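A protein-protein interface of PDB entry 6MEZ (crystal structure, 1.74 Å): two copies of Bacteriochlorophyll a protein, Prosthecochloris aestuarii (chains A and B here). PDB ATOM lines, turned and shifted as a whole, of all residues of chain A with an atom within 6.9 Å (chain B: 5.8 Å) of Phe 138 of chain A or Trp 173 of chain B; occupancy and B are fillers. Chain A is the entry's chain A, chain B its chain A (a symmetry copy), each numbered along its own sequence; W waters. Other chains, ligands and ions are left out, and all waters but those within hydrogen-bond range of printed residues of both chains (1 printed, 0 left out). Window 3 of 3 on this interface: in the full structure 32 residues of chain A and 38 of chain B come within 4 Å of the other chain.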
ATOM      1  N   SER A 111     -28.081  24.515  11.177  1.00  0.00           N
ATOM      2  CA  SER A 111     -27.139  23.416  11.324  1.00  0.00           C
ATOM      3  C   SER A 111     -25.835  23.809  10.664  1.00  0.00           C
ATOM      4  O   SER A 111     -25.815  24.562   9.681  1.00  0.00           O
ATOM      5  CB  SER A 111     -27.698  22.115  10.735  1.00  0.00           C
ATOM      6  OG  SER A 111     -27.913  22.213   9.342  1.00  0.00           O
ATOM      7  N   VAL A 112     -24.744  23.343  11.247  1.00  0.00           N
ATOM      8  CA  VAL A 112     -23.422  23.595  10.683  1.00  0.00           C
ATOM      9  C   VAL A 112     -22.696  22.264  10.623  1.00  0.00           C
ATOM     10  O   VAL A 112     -22.661  21.523  11.609  1.00  0.00           O
ATOM     11  CB  VAL A 112     -22.623  24.604  11.516  1.00  0.00           C
ATOM     12  CG1 VAL A 112     -21.247  24.806  10.920  1.00  0.00           C
ATOM     13  CG2 VAL A 112     -23.350  25.942  11.597  1.00  0.00           C
ATOM     14  N   VAL A 113     -22.134  21.949   9.464  1.00  0.00           N
ATOM     15  CA  VAL A 113     -21.393  20.705   9.304  1.00  0.00           C
ATOM     16  C   VAL A 113     -19.952  21.036   8.958  1.00  0.00           C
ATOM     17  O   VAL A 113     -19.694  21.723   7.979  1.00  0.00           O
ATOM     18  CB  VAL A 113     -21.979  19.810   8.199  1.00  0.00           C
ATOM     19  CG1 VAL A 113     -21.086  18.605   7.991  1.00  0.00           C
ATOM     20  CG2 VAL A 113     -23.404  19.374   8.553  1.00  0.00           C
ATOM     21  N   ASN A 114     -19.021  20.529   9.755  1.00  0.00           N
ATOM     22  CA  ASN A 114     -17.601  20.749   9.511  1.00  0.00           C
ATOM     23  C   ASN A 114     -17.008  19.585   8.751  1.00  0.00           C
ATOM     24  O   ASN A 114     -17.229  18.431   9.107  1.00  0.00           O
ATOM     25  CB  ASN A 114     -16.845  20.928  10.829  1.00  0.00           C
ATOM     26  CG  ASN A 114     -15.475  21.530  10.619  1.00  0.00           C
ATOM     27  OD1 ASN A 114     -15.364  22.697  10.252  1.00  0.00           O
ATOM     28  ND2 ASN A 114     -14.439  20.738  10.820  1.00  0.00           N
ATOM     29  N   MET A 115     -16.274  19.867   7.680  1.00  0.00           N
ATOM     30  CA  MET A 115     -15.640  18.796   6.919  1.00  0.00           C
ATOM     31  C   MET A 115     -14.164  19.068   6.669  1.00  0.00           C
ATOM     32  O   MET A 115     -13.802  20.012   5.973  1.00  0.00           O
ATOM     33  CB  MET A 115     -16.346  18.587   5.578  1.00  0.00           C
ATOM     34  CG  MET A 115     -15.743  17.460   4.742  1.00  0.00           C
ATOM     35  SD  MET A 115     -16.333  17.496   3.034  1.00  0.00           S
ATOM     36  CE  MET A 115     -15.529  18.979   2.417  1.00  0.00           C
ATOM     37  N   TYR A 117     -10.631  18.266   4.905  1.00  0.00           N
ATOM     38  CA  TYR A 117     -10.256  17.744   3.638  1.00  0.00           C
ATOM     39  C   TYR A 117      -9.169  16.679   3.830  1.00  0.00           C
ATOM     40  O   TYR A 117      -8.181  16.931   4.439  1.00  0.00           O
ATOM     41  CB  TYR A 117      -9.650  18.845   2.762  1.00  0.00           C
ATOM     42  CG  TYR A 117     -10.537  19.969   2.275  1.00  0.00           C
ATOM     43  CD1 TYR A 117     -11.735  19.742   1.673  1.00  0.00           C
ATOM     44  CD2 TYR A 117     -10.121  21.243   2.339  1.00  0.00           C
ATOM     45  CE1 TYR A 117     -12.513  20.775   1.209  1.00  0.00           C
ATOM     46  CE2 TYR A 117     -10.884  22.274   1.893  1.00  0.00           C
ATOM     47  CZ  TYR A 117     -12.085  22.035   1.295  1.00  0.00           C
ATOM     48  OH  TYR A 117     -12.823  23.071   0.845  1.00  0.00           O
ATOM     49  N   TYR A 118      -9.383  15.524   3.293  1.00  0.00           N
ATOM     50  CA  TYR A 118      -8.382  14.498   3.283  1.00  0.00           C
ATOM     51  C   TYR A 118      -7.492  14.245   4.500  1.00  0.00           C
ATOM     52  O   TYR A 118      -6.269  14.351   4.412  1.00  0.00           O
ATOM     53  CB  TYR A 118      -7.518  14.737   2.050  1.00  0.00           C
ATOM     54  CG  TYR A 118      -8.299  15.152   0.806  1.00  0.00           C
ATOM     55  CD1 TYR A 118      -9.129  14.274   0.173  1.00  0.00           C
ATOM     56  CD2 TYR A 118      -8.242  16.444   0.321  1.00  0.00           C
ATOM     57  CE1 TYR A 118      -9.856  14.658  -0.912  1.00  0.00           C
ATOM     58  CE2 TYR A 118      -8.964  16.832  -0.758  1.00  0.00           C
ATOM     59  CZ  TYR A 118      -9.770  15.928  -1.370  1.00  0.00           C
ATOM     60  OH  TYR A 118     -10.502  16.289  -2.438  1.00  0.00           O
ATOM     61  N   ARG A 136     -13.778  22.748   5.045  1.00  0.00           N
ATOM     62  CA  ARG A 136     -14.889  23.572   4.608  1.00  0.00           C
ATOM     63  C   ARG A 136     -16.052  23.301   5.544  1.00  0.00           C
ATOM     64  O   ARG A 136     -16.194  22.190   6.050  1.00  0.00           O
ATOM     65  CB  ARG A 136     -15.263  23.257   3.147  1.00  0.00           C
ATOM     66  CG  ARG A 136     -16.416  24.117   2.581  1.00  0.00           C
ATOM     67  CD  ARG A 136     -16.514  23.972   1.047  1.00  0.00           C
ATOM     68  NE  ARG A 136     -15.415  24.656   0.352  1.00  0.00           N
ATOM     69  CZ  ARG A 136     -15.478  25.907  -0.107  1.00  0.00           C
ATOM     70  NH1 ARG A 136     -16.584  26.634   0.069  1.00  0.00           N
ATOM     71  NH2 ARG A 136     -14.431  26.451  -0.727  1.00  0.00           N
ATOM     72  N   GLN A 137     -16.881  24.314   5.770  1.00  0.00           N
ATOM     73  CA  GLN A 137     -17.883  24.271   6.834  1.00  0.00           C
ATOM     74  C   GLN A 137     -19.213  24.783   6.311  1.00  0.00           C
ATOM     75  O   GLN A 137     -19.308  25.954   5.932  1.00  0.00           O
ATOM     76  CB  GLN A 137     -17.404  25.126   8.009  1.00  0.00           C
ATOM     77  CG  GLN A 137     -18.262  25.059   9.248  1.00  0.00           C
ATOM     78  CD  GLN A 137     -17.591  25.793  10.382  1.00  0.00           C
ATOM     79  OE1 GLN A 137     -17.950  26.927  10.694  1.00  0.00           O
ATOM     80  NE2 GLN A 137     -16.580  25.161  10.979  1.00  0.00           N
ATOM     81  N   PHE A 138     -20.232  23.921   6.299  1.00  0.00           N
ATOM     82  CA  PHE A 138     -21.505  24.220   5.630  1.00  0.00           C
ATOM     83  C   PHE A 138     -22.586  24.693   6.585  1.00  0.00           C
ATOM     84  O   PHE A 138     -22.898  24.009   7.557  1.00  0.00           O
ATOM     85  CB  PHE A 138     -21.993  22.971   4.882  1.00  0.00           C
ATOM     86  CG  PHE A 138     -20.993  22.452   3.884  1.00  0.00           C
ATOM     87  CD1 PHE A 138     -19.985  21.575   4.268  1.00  0.00           C
ATOM     88  CD2 PHE A 138     -21.055  22.856   2.563  1.00  0.00           C
ATOM     89  CE1 PHE A 138     -19.048  21.112   3.343  1.00  0.00           C
ATOM     90  CE2 PHE A 138     -20.121  22.397   1.635  1.00  0.00           C
ATOM     91  CZ  PHE A 138     -19.120  21.524   2.027  1.00  0.00           C
ATOM     92  N   HIS A 139     -23.190  25.830   6.289  1.00  0.00           N
ATOM     93  CA  HIS A 139     -24.245  26.379   7.085  1.00  0.00           C
ATOM     94  C   HIS A 139     -25.611  26.222   6.395  1.00  0.00           C
ATOM     95  O   HIS A 139     -25.722  26.474   5.253  1.00  0.00           O
ATOM     96  CB  HIS A 139     -24.031  27.870   7.269  1.00  0.00           C
ATOM     97  CG  HIS A 139     -23.049  28.216   8.333  1.00  0.00           C
ATOM     98  ND1 HIS A 139     -21.744  27.810   8.284  1.00  0.00           N
ATOM     99  CD2 HIS A 139     -23.166  28.954   9.458  1.00  0.00           C
ATOM    100  CE1 HIS A 139     -21.107  28.266   9.338  1.00  0.00           C
ATOM    101  NE2 HIS A 139     -21.939  28.981  10.052  1.00  0.00           N
ATOM    102  N   ASP A 140     -26.607  25.808   7.149  1.00  0.00           N
ATOM    103  CA  ASP A 140     -27.988  25.691   6.690  1.00  0.00           C
ATOM    104  C   ASP A 140     -28.850  26.452   7.692  1.00  0.00           C
ATOM    105  O   ASP A 140     -28.926  26.062   8.856  1.00  0.00           O
ATOM    106  CB  ASP A 140     -28.402  24.226   6.610  1.00  0.00           C
ATOM    107  CG  ASP A 140     -29.760  24.012   5.940  1.00  0.00           C
ATOM    108  OD1 ASP A 140     -30.076  22.842   5.649  1.00  0.00           O
ATOM    109  OD2 ASP A 140     -30.498  24.983   5.676  1.00  0.00           O
ATOM    110  N   ARG A 193     -12.255  31.535   2.653  1.00  0.00           N
ATOM    111  CA  ARG A 193     -13.100  31.719   1.467  1.00  0.00           C
ATOM    112  C   ARG A 193     -14.552  31.667   1.886  1.00  0.00           C
ATOM    113  O   ARG A 193     -14.910  30.846   2.715  1.00  0.00           O
ATOM    114  CB  ARG A 193     -12.852  30.629   0.429  1.00  0.00           C
ATOM    115  CG  ARG A 193     -11.413  30.507  -0.029  1.00  0.00           C
ATOM    116  CD  ARG A 193     -11.286  29.431  -1.116  1.00  0.00           C
ATOM    117  NE  ARG A 193     -12.037  29.791  -2.321  1.00  0.00           N
ATOM    118  CZ  ARG A 193     -12.302  28.948  -3.315  1.00  0.00           C
ATOM    119  NH1 ARG A 193     -11.903  27.688  -3.245  1.00  0.00           N
ATOM    120  NH2 ARG A 193     -12.985  29.353  -4.377  1.00  0.00           N
ATOM    121  N   SER A 195     -18.377  31.115   0.261  1.00  0.00           N
ATOM    122  CA  SER A 195     -19.077  30.729  -0.952  1.00  0.00           C
ATOM    123  C   SER A 195     -20.184  31.724  -1.261  1.00  0.00           C
ATOM    124  O   SER A 195     -20.632  32.455  -0.376  1.00  0.00           O
ATOM    125  CB  SER A 195     -19.689  29.330  -0.813  1.00  0.00           C
ATOM    126  OG  SER A 195     -20.861  29.395  -0.011  1.00  0.00           O
ATOM    127  N   LYS A 218     -28.317  29.024   2.574  1.00  0.00           N
ATOM    128  CA  LYS A 218     -27.147  28.196   2.822  1.00  0.00           C
ATOM    129  C   LYS A 218     -25.909  28.921   2.349  1.00  0.00           C
ATOM    130  O   LYS A 218     -25.976  29.701   1.398  1.00  0.00           O
ATOM    131  CB  LYS A 218     -27.234  26.860   2.071  1.00  0.00           C
ATOM    132  CG  LYS A 218     -28.345  25.925   2.466  1.00  0.00           C
ATOM    133  CD  LYS A 218     -28.355  24.738   1.492  1.00  0.00           C
ATOM    134  CE  LYS A 218     -29.016  23.508   2.107  1.00  0.00           C
ATOM    135  NZ  LYS A 218     -30.388  23.788   2.627  1.00  0.00           N
ATOM    136  N   PHE A 219     -24.780  28.657   3.002  1.00  0.00           N
ATOM    137  CA  PHE A 219     -23.479  29.055   2.463  1.00  0.00           C
ATOM    138  C   PHE A 219     -22.435  28.142   3.066  1.00  0.00           C
ATOM    139  O   PHE A 219     -22.699  27.460   4.052  1.00  0.00           O
ATOM    140  CB  PHE A 219     -23.141  30.522   2.773  1.00  0.00           C
ATOM    141  CG  PHE A 219     -22.773  30.782   4.217  1.00  0.00           C
ATOM    142  CD1 PHE A 219     -21.435  30.827   4.615  1.00  0.00           C
ATOM    143  CD2 PHE A 219     -23.756  31.033   5.171  1.00  0.00           C
ATOM    144  CE1 PHE A 219     -21.097  31.074   5.954  1.00  0.00           C
ATOM    145  CE2 PHE A 219     -23.420  31.288   6.503  1.00  0.00           C
ATOM    146  CZ  PHE A 219     -22.088  31.307   6.888  1.00  0.00           C
ATOM    147  N   SER A 220     -21.236  28.139   2.507  1.00  0.00           N
ATOM    148  CA  SER A 220     -20.130  27.488   3.195  1.00  0.00           C
ATOM    149  C   SER A 220     -18.954  28.446   3.286  1.00  0.00           C
ATOM    150  O   SER A 220     -18.857  29.421   2.523  1.00  0.00           O
ATOM    151  CB  SER A 220     -19.725  26.177   2.501  1.00  0.00           C
ATOM    152  OG  SER A 220     -19.270  26.385   1.170  1.00  0.00           O
ATOM    153  N   HIS A 221     -18.070  28.200   4.241  1.00  0.00           N
ATOM    154  CA  HIS A 221     -16.800  28.925   4.229  1.00  0.00           C
ATOM    155  C   HIS A 221     -15.696  27.890   4.363  1.00  0.00           C
ATOM    156  O   HIS A 221     -15.933  26.776   4.846  1.00  0.00           O
ATOM    157  CB  HIS A 221     -16.753  30.015   5.331  1.00  0.00           C
ATOM    158  CG  HIS A 221     -16.637  29.494   6.732  1.00  0.00           C
ATOM    159  ND1 HIS A 221     -15.536  29.750   7.524  1.00  0.00           N
ATOM    160  CD2 HIS A 221     -17.488  28.758   7.490  1.00  0.00           C
ATOM    161  CE1 HIS A 221     -15.702  29.170   8.702  1.00  0.00           C
ATOM    162  NE2 HIS A 221     -16.881  28.571   8.710  1.00  0.00           N
ATOM    163  N   ALA A 222     -14.506  28.223   3.876  1.00  0.00           N
ATOM    164  CA  ALA A 222     -13.408  27.264   3.868  1.00  0.00           C
ATOM    165  C   ALA A 222     -12.143  27.929   4.387  1.00  0.00           C
ATOM    166  O   ALA A 222     -12.051  29.157   4.430  1.00  0.00           O
ATOM    167  CB  ALA A 222     -13.175  26.709   2.463  1.00  0.00           C
ATOM    168  N   ALA B 168     -17.342  19.875 -10.334  1.00  0.00           N
ATOM    169  CA  ALA B 168     -16.513  21.073 -10.514  1.00  0.00           C
ATOM    170  C   ALA B 168     -15.928  21.555  -9.198  1.00  0.00           C
ATOM    171  O   ALA B 168     -14.917  22.284  -9.178  1.00  0.00           O
ATOM    172  CB  ALA B 168     -17.318  22.187 -11.161  1.00  0.00           C
ATOM    173  N   ASN B 169     -16.558  21.149  -8.099  1.00  0.00           N
ATOM    174  CA  ASN B 169     -16.083  21.554  -6.782  1.00  0.00           C
ATOM    175  C   ASN B 169     -14.678  21.042  -6.483  1.00  0.00           C
ATOM    176  O   ASN B 169     -13.902  21.729  -5.836  1.00  0.00           O
ATOM    177  CB  ASN B 169     -17.047  21.081  -5.688  1.00  0.00           C
ATOM    178  CG  ASN B 169     -18.351  21.853  -5.688  1.00  0.00           C
ATOM    179  OD1 ASN B 169     -18.447  22.923  -6.280  1.00  0.00           O
ATOM    180  ND2 ASN B 169     -19.358  21.311  -5.025  1.00  0.00           N
ATOM    181  N   PHE B 170     -14.345  19.839  -6.946  1.00  0.00           N
ATOM    182  CA  PHE B 170     -13.063  19.262  -6.572  1.00  0.00           C
ATOM    183  C   PHE B 170     -11.889  20.151  -6.976  1.00  0.00           C
ATOM    184  O   PHE B 170     -11.029  20.437  -6.158  1.00  0.00           O
ATOM    185  CB  PHE B 170     -12.853  17.878  -7.183  1.00  0.00           C
ATOM    186  CG  PHE B 170     -11.466  17.367  -6.982  1.00  0.00           C
ATOM    187  CD1 PHE B 170     -11.083  16.829  -5.761  1.00  0.00           C
ATOM    188  CD2 PHE B 170     -10.518  17.468  -7.990  1.00  0.00           C
ATOM    189  CE1 PHE B 170      -9.780  16.384  -5.558  1.00  0.00           C
ATOM    190  CE2 PHE B 170      -9.227  17.012  -7.793  1.00  0.00           C
ATOM    191  CZ  PHE B 170      -8.859  16.474  -6.575  1.00  0.00           C
ATOM    192  N   GLY B 171     -11.857  20.576  -8.237  1.00  0.00           N
ATOM    193  CA  GLY B 171     -10.718  21.347  -8.732  1.00  0.00           C
ATOM    194  C   GLY B 171     -10.671  22.782  -8.218  1.00  0.00           C
ATOM    195  O   GLY B 171      -9.645  23.443  -8.297  1.00  0.00           O
ATOM    196  N   ASP B 172     -11.799  23.239  -7.691  1.00  0.00           N
ATOM    197  CA  ASP B 172     -11.957  24.557  -7.096  1.00  0.00           C
ATOM    198  C   ASP B 172     -11.458  24.501  -5.642  1.00  0.00           C
ATOM    199  O   ASP B 172     -10.468  25.151  -5.271  1.00  0.00           O
ATOM    200  CB  ASP B 172     -13.441  24.946  -7.183  1.00  0.00           C
ATOM    201  CG  ASP B 172     -13.760  26.297  -6.557  1.00  0.00           C
ATOM    202  OD1 ASP B 172     -12.887  26.923  -5.934  1.00  0.00           O
ATOM    203  OD2 ASP B 172     -14.934  26.707  -6.682  1.00  0.00           O
ATOM    204  N   TRP B 173     -12.124  23.676  -4.845  1.00  0.00           N
ATOM    205  CA  TRP B 173     -11.816  23.562  -3.420  1.00  0.00           C
ATOM    206  C   TRP B 173     -10.458  22.994  -3.084  1.00  0.00           C
ATOM    207  O   TRP B 173      -9.976  23.171  -1.959  1.00  0.00           O
ATOM    208  CB  TRP B 173     -12.865  22.692  -2.721  1.00  0.00           C
ATOM    209  CG  TRP B 173     -14.256  23.254  -2.748  1.00  0.00           C
ATOM    210  CD1 TRP B 173     -14.654  24.474  -3.214  1.00  0.00           C
ATOM    211  CD2 TRP B 173     -15.436  22.577  -2.322  1.00  0.00           C
ATOM    212  NE1 TRP B 173     -16.021  24.605  -3.086  1.00  0.00           N
ATOM    213  CE2 TRP B 173     -16.524  23.452  -2.539  1.00  0.00           C
ATOM    214  CE3 TRP B 173     -15.680  21.318  -1.763  1.00  0.00           C
ATOM    215  CZ2 TRP B 173     -17.842  23.107  -2.212  1.00  0.00           C
ATOM    216  CZ3 TRP B 173     -16.995  20.975  -1.436  1.00  0.00           C
ATOM    217  CH2 TRP B 173     -18.053  21.866  -1.668  1.00  0.00           C
ATOM    218  N   ILE B 174      -9.812  22.307  -4.023  1.00  0.00           N
ATOM    219  CA  ILE B 174      -8.483  21.775  -3.758  1.00  0.00           C
ATOM    220  C   ILE B 174      -7.485  22.894  -3.475  1.00  0.00           C
ATOM    221  O   ILE B 174      -6.449  22.667  -2.859  1.00  0.00           O
ATOM    222  CB  ILE B 174      -7.968  20.907  -4.939  1.00  0.00           C
ATOM    223  CG1 ILE B 174      -6.777  20.043  -4.515  1.00  0.00           C
ATOM    224  CG2 ILE B 174      -7.619  21.775  -6.142  1.00  0.00           C
ATOM    225  CD1 ILE B 174      -7.130  18.949  -3.511  1.00  0.00           C
ATOM    226  N   ARG B 175      -7.794  24.122  -3.894  1.00  0.00           N
ATOM    227  CA  ARG B 175      -6.799  25.176  -3.756  1.00  0.00           C
ATOM    228  C   ARG B 175      -6.534  25.557  -2.297  1.00  0.00           C
ATOM    229  O   ARG B 175      -5.391  25.820  -1.931  1.00  0.00           O
ATOM    230  CB  ARG B 175      -7.209  26.404  -4.580  1.00  0.00           C
ATOM    231  CG  ARG B 175      -7.051  26.113  -6.076  1.00  0.00           C
ATOM    232  CD  ARG B 175      -7.545  27.242  -6.954  1.00  0.00           C
ATOM    233  NE  ARG B 175      -8.996  27.359  -6.907  1.00  0.00           N
ATOM    234  CZ  ARG B 175      -9.675  28.264  -7.593  1.00  0.00           C
ATOM    235  NH1 ARG B 175      -9.008  29.115  -8.372  1.00  0.00           N
ATOM    236  NH2 ARG B 175     -11.001  28.306  -7.525  1.00  0.00           N
ATOM    237  N   GLU B 176      -7.545  25.528  -1.445  1.00  0.00           N
ATOM    238  CA  GLU B 176      -7.266  25.838  -0.036  1.00  0.00           C
ATOM    239  C   GLU B 176      -6.643  24.648   0.706  1.00  0.00           C
ATOM    240  O   GLU B 176      -6.108  24.815   1.795  1.00  0.00           O
ATOM    241  CB  GLU B 176      -8.523  26.320   0.695  1.00  0.00           C
ATOM    242  CG  GLU B 176      -9.693  25.371   0.690  1.00  0.00           C
ATOM    243  CD  GLU B 176     -10.673  25.656  -0.443  1.00  0.00           C
ATOM    244  OE1 GLU B 176     -10.266  26.265  -1.452  1.00  0.00           O
ATOM    245  OE2 GLU B 176     -11.848  25.260  -0.326  1.00  0.00           O
ATOM    246  N   PHE B 177      -6.697  23.454   0.122  1.00  0.00           N
ATOM    247  CA  PHE B 177      -5.952  22.312   0.663  1.00  0.00           C
ATOM    248  C   PHE B 177      -4.469  22.413   0.293  1.00  0.00           C
ATOM    249  O   PHE B 177      -3.576  22.245   1.117  1.00  0.00           O
ATOM    250  CB  PHE B 177      -6.544  20.990   0.138  1.00  0.00           C
ATOM    251  CG  PHE B 177      -5.764  19.761   0.561  1.00  0.00           C
ATOM    252  CD1 PHE B 177      -4.891  19.149  -0.311  1.00  0.00           C
ATOM    253  CD2 PHE B 177      -5.918  19.230   1.834  1.00  0.00           C
ATOM    254  CE1 PHE B 177      -4.178  18.029   0.066  1.00  0.00           C
ATOM    255  CE2 PHE B 177      -5.209  18.106   2.220  1.00  0.00           C
ATOM    256  CZ  PHE B 177      -4.325  17.514   1.325  1.00  0.00           C
HETATM  257  O   HOH W   1     -11.044  19.084  -3.192  1.00  0.00           O
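OD1 of Asp 172 of chain B is in salt-bridge range of NH2 of Arg 175 of chain B. N of Met 115 of chain A lies within hydrogen-bond range of O of Arg 136 of chain A, at 2.8 Å. NH1 of Arg 136 of chain A sits at hydrogen-bond distance from OG of Ser 220 of chain A, 2.9 Å away. OH of Tyr 117 of chain A sits at hydrogen-bond distance from NE of Arg 136 of chain A (3.1 Å). N of Ala 222 of chain A lies within hydrogen-bond range of O of Arg 193 of chain A, 2.9 Å away. N of Phe 138 of chain A lies within hydrogen-bond range of O of Val 113 of chain A.
No position is printed for both chains. Of the 13 pairs that touch across the chains among the printed residues, none has its exchanged pair printed and touching as well.
Of the 19 printed residues of chain A, 6 touch a printed residue of chain B. Printed residues of chain A that touch a printed residue of chain B: Tyr 117, Tyr 118, Arg 136, Phe 138, Arg 193 and Ala 222.
NH2 of Arg 193 of chain A lies within salt-bridge range of OD1 of Asp 172 of chain B (2.9 Å). The guanidinium group of Arg 136 of chain A sits close to the indole nitrogen of Trp 173 of chain B. The side-chain carboxylate of Glu 176 of chain B is in salt-bridge range of the guanidinium group of Arg 193 of chain A (2.8 Å). NH2 of Arg 136 of chain A lies within salt-bridge range of OE2 of Glu 176 of chain B. OE2 of Glu 176 of chain B lies within hydrogen-bond range of OH of Tyr 117 of chain A (2.7 Å).
Of chain B, only Trp 173 comes within 4 Å of Phe 138 of chain A. Trp 173 of chain B touches just these residues of chain A: Tyr 117, Arg 136 and Phe 138. Printed residues of chain B within 4 Å of Arg 193 of chain A: Asp 172 (2.9 Å), Arg 175 (3.9 Å) and Glu 176 (2.8 Å). Of the printed residues of chain A, Asp 172 of chain B touches Arg 193. Printed residues of chain B within 4 Å of Arg 136 of chain A: Trp 173 and Glu 176. Lys 218 of chain A touches none of the printed residues of chain B. The nearest printed residue of chain B that does not touch Phe 138 of chain A is Asn 169 of chain B (6.8 Å). The nearest residue of chain A that does not touch Trp 173 of chain B is Arg 193 of chain A (4.1 Å).
Water W1 lies within hydrogen-bond range of OH of Tyr 118 of chain A (2.9 Å) and O of Phe 170 of chain B (3.3 Å).
Tyr 117 of chain A touches Trp 173 of chain B (OH to CB, 3.6 Å). CD2 of Phe 177 of chain B touches CB of Tyr 117 of chain A, 3.9 Å away. Phe 170 of chain B touches Tyr 118 of chain A (CE1 to OH, 3.2 Å). Tyr 118 of chain A touches Ile 174 of chain B. CD2 of Tyr 118 of chain A touches CD2 of Phe 177 of chain B, 3.9 Å away. CZ of Phe 138 of chain A touches CH2 of Trp 173 of chain B, 3.9 Å away. Arg 175 of chain B touches Arg 193 of chain A (NH2 to NH2, 3.9 Å). Ala 222 of chain A touches Glu 176 of chain B.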
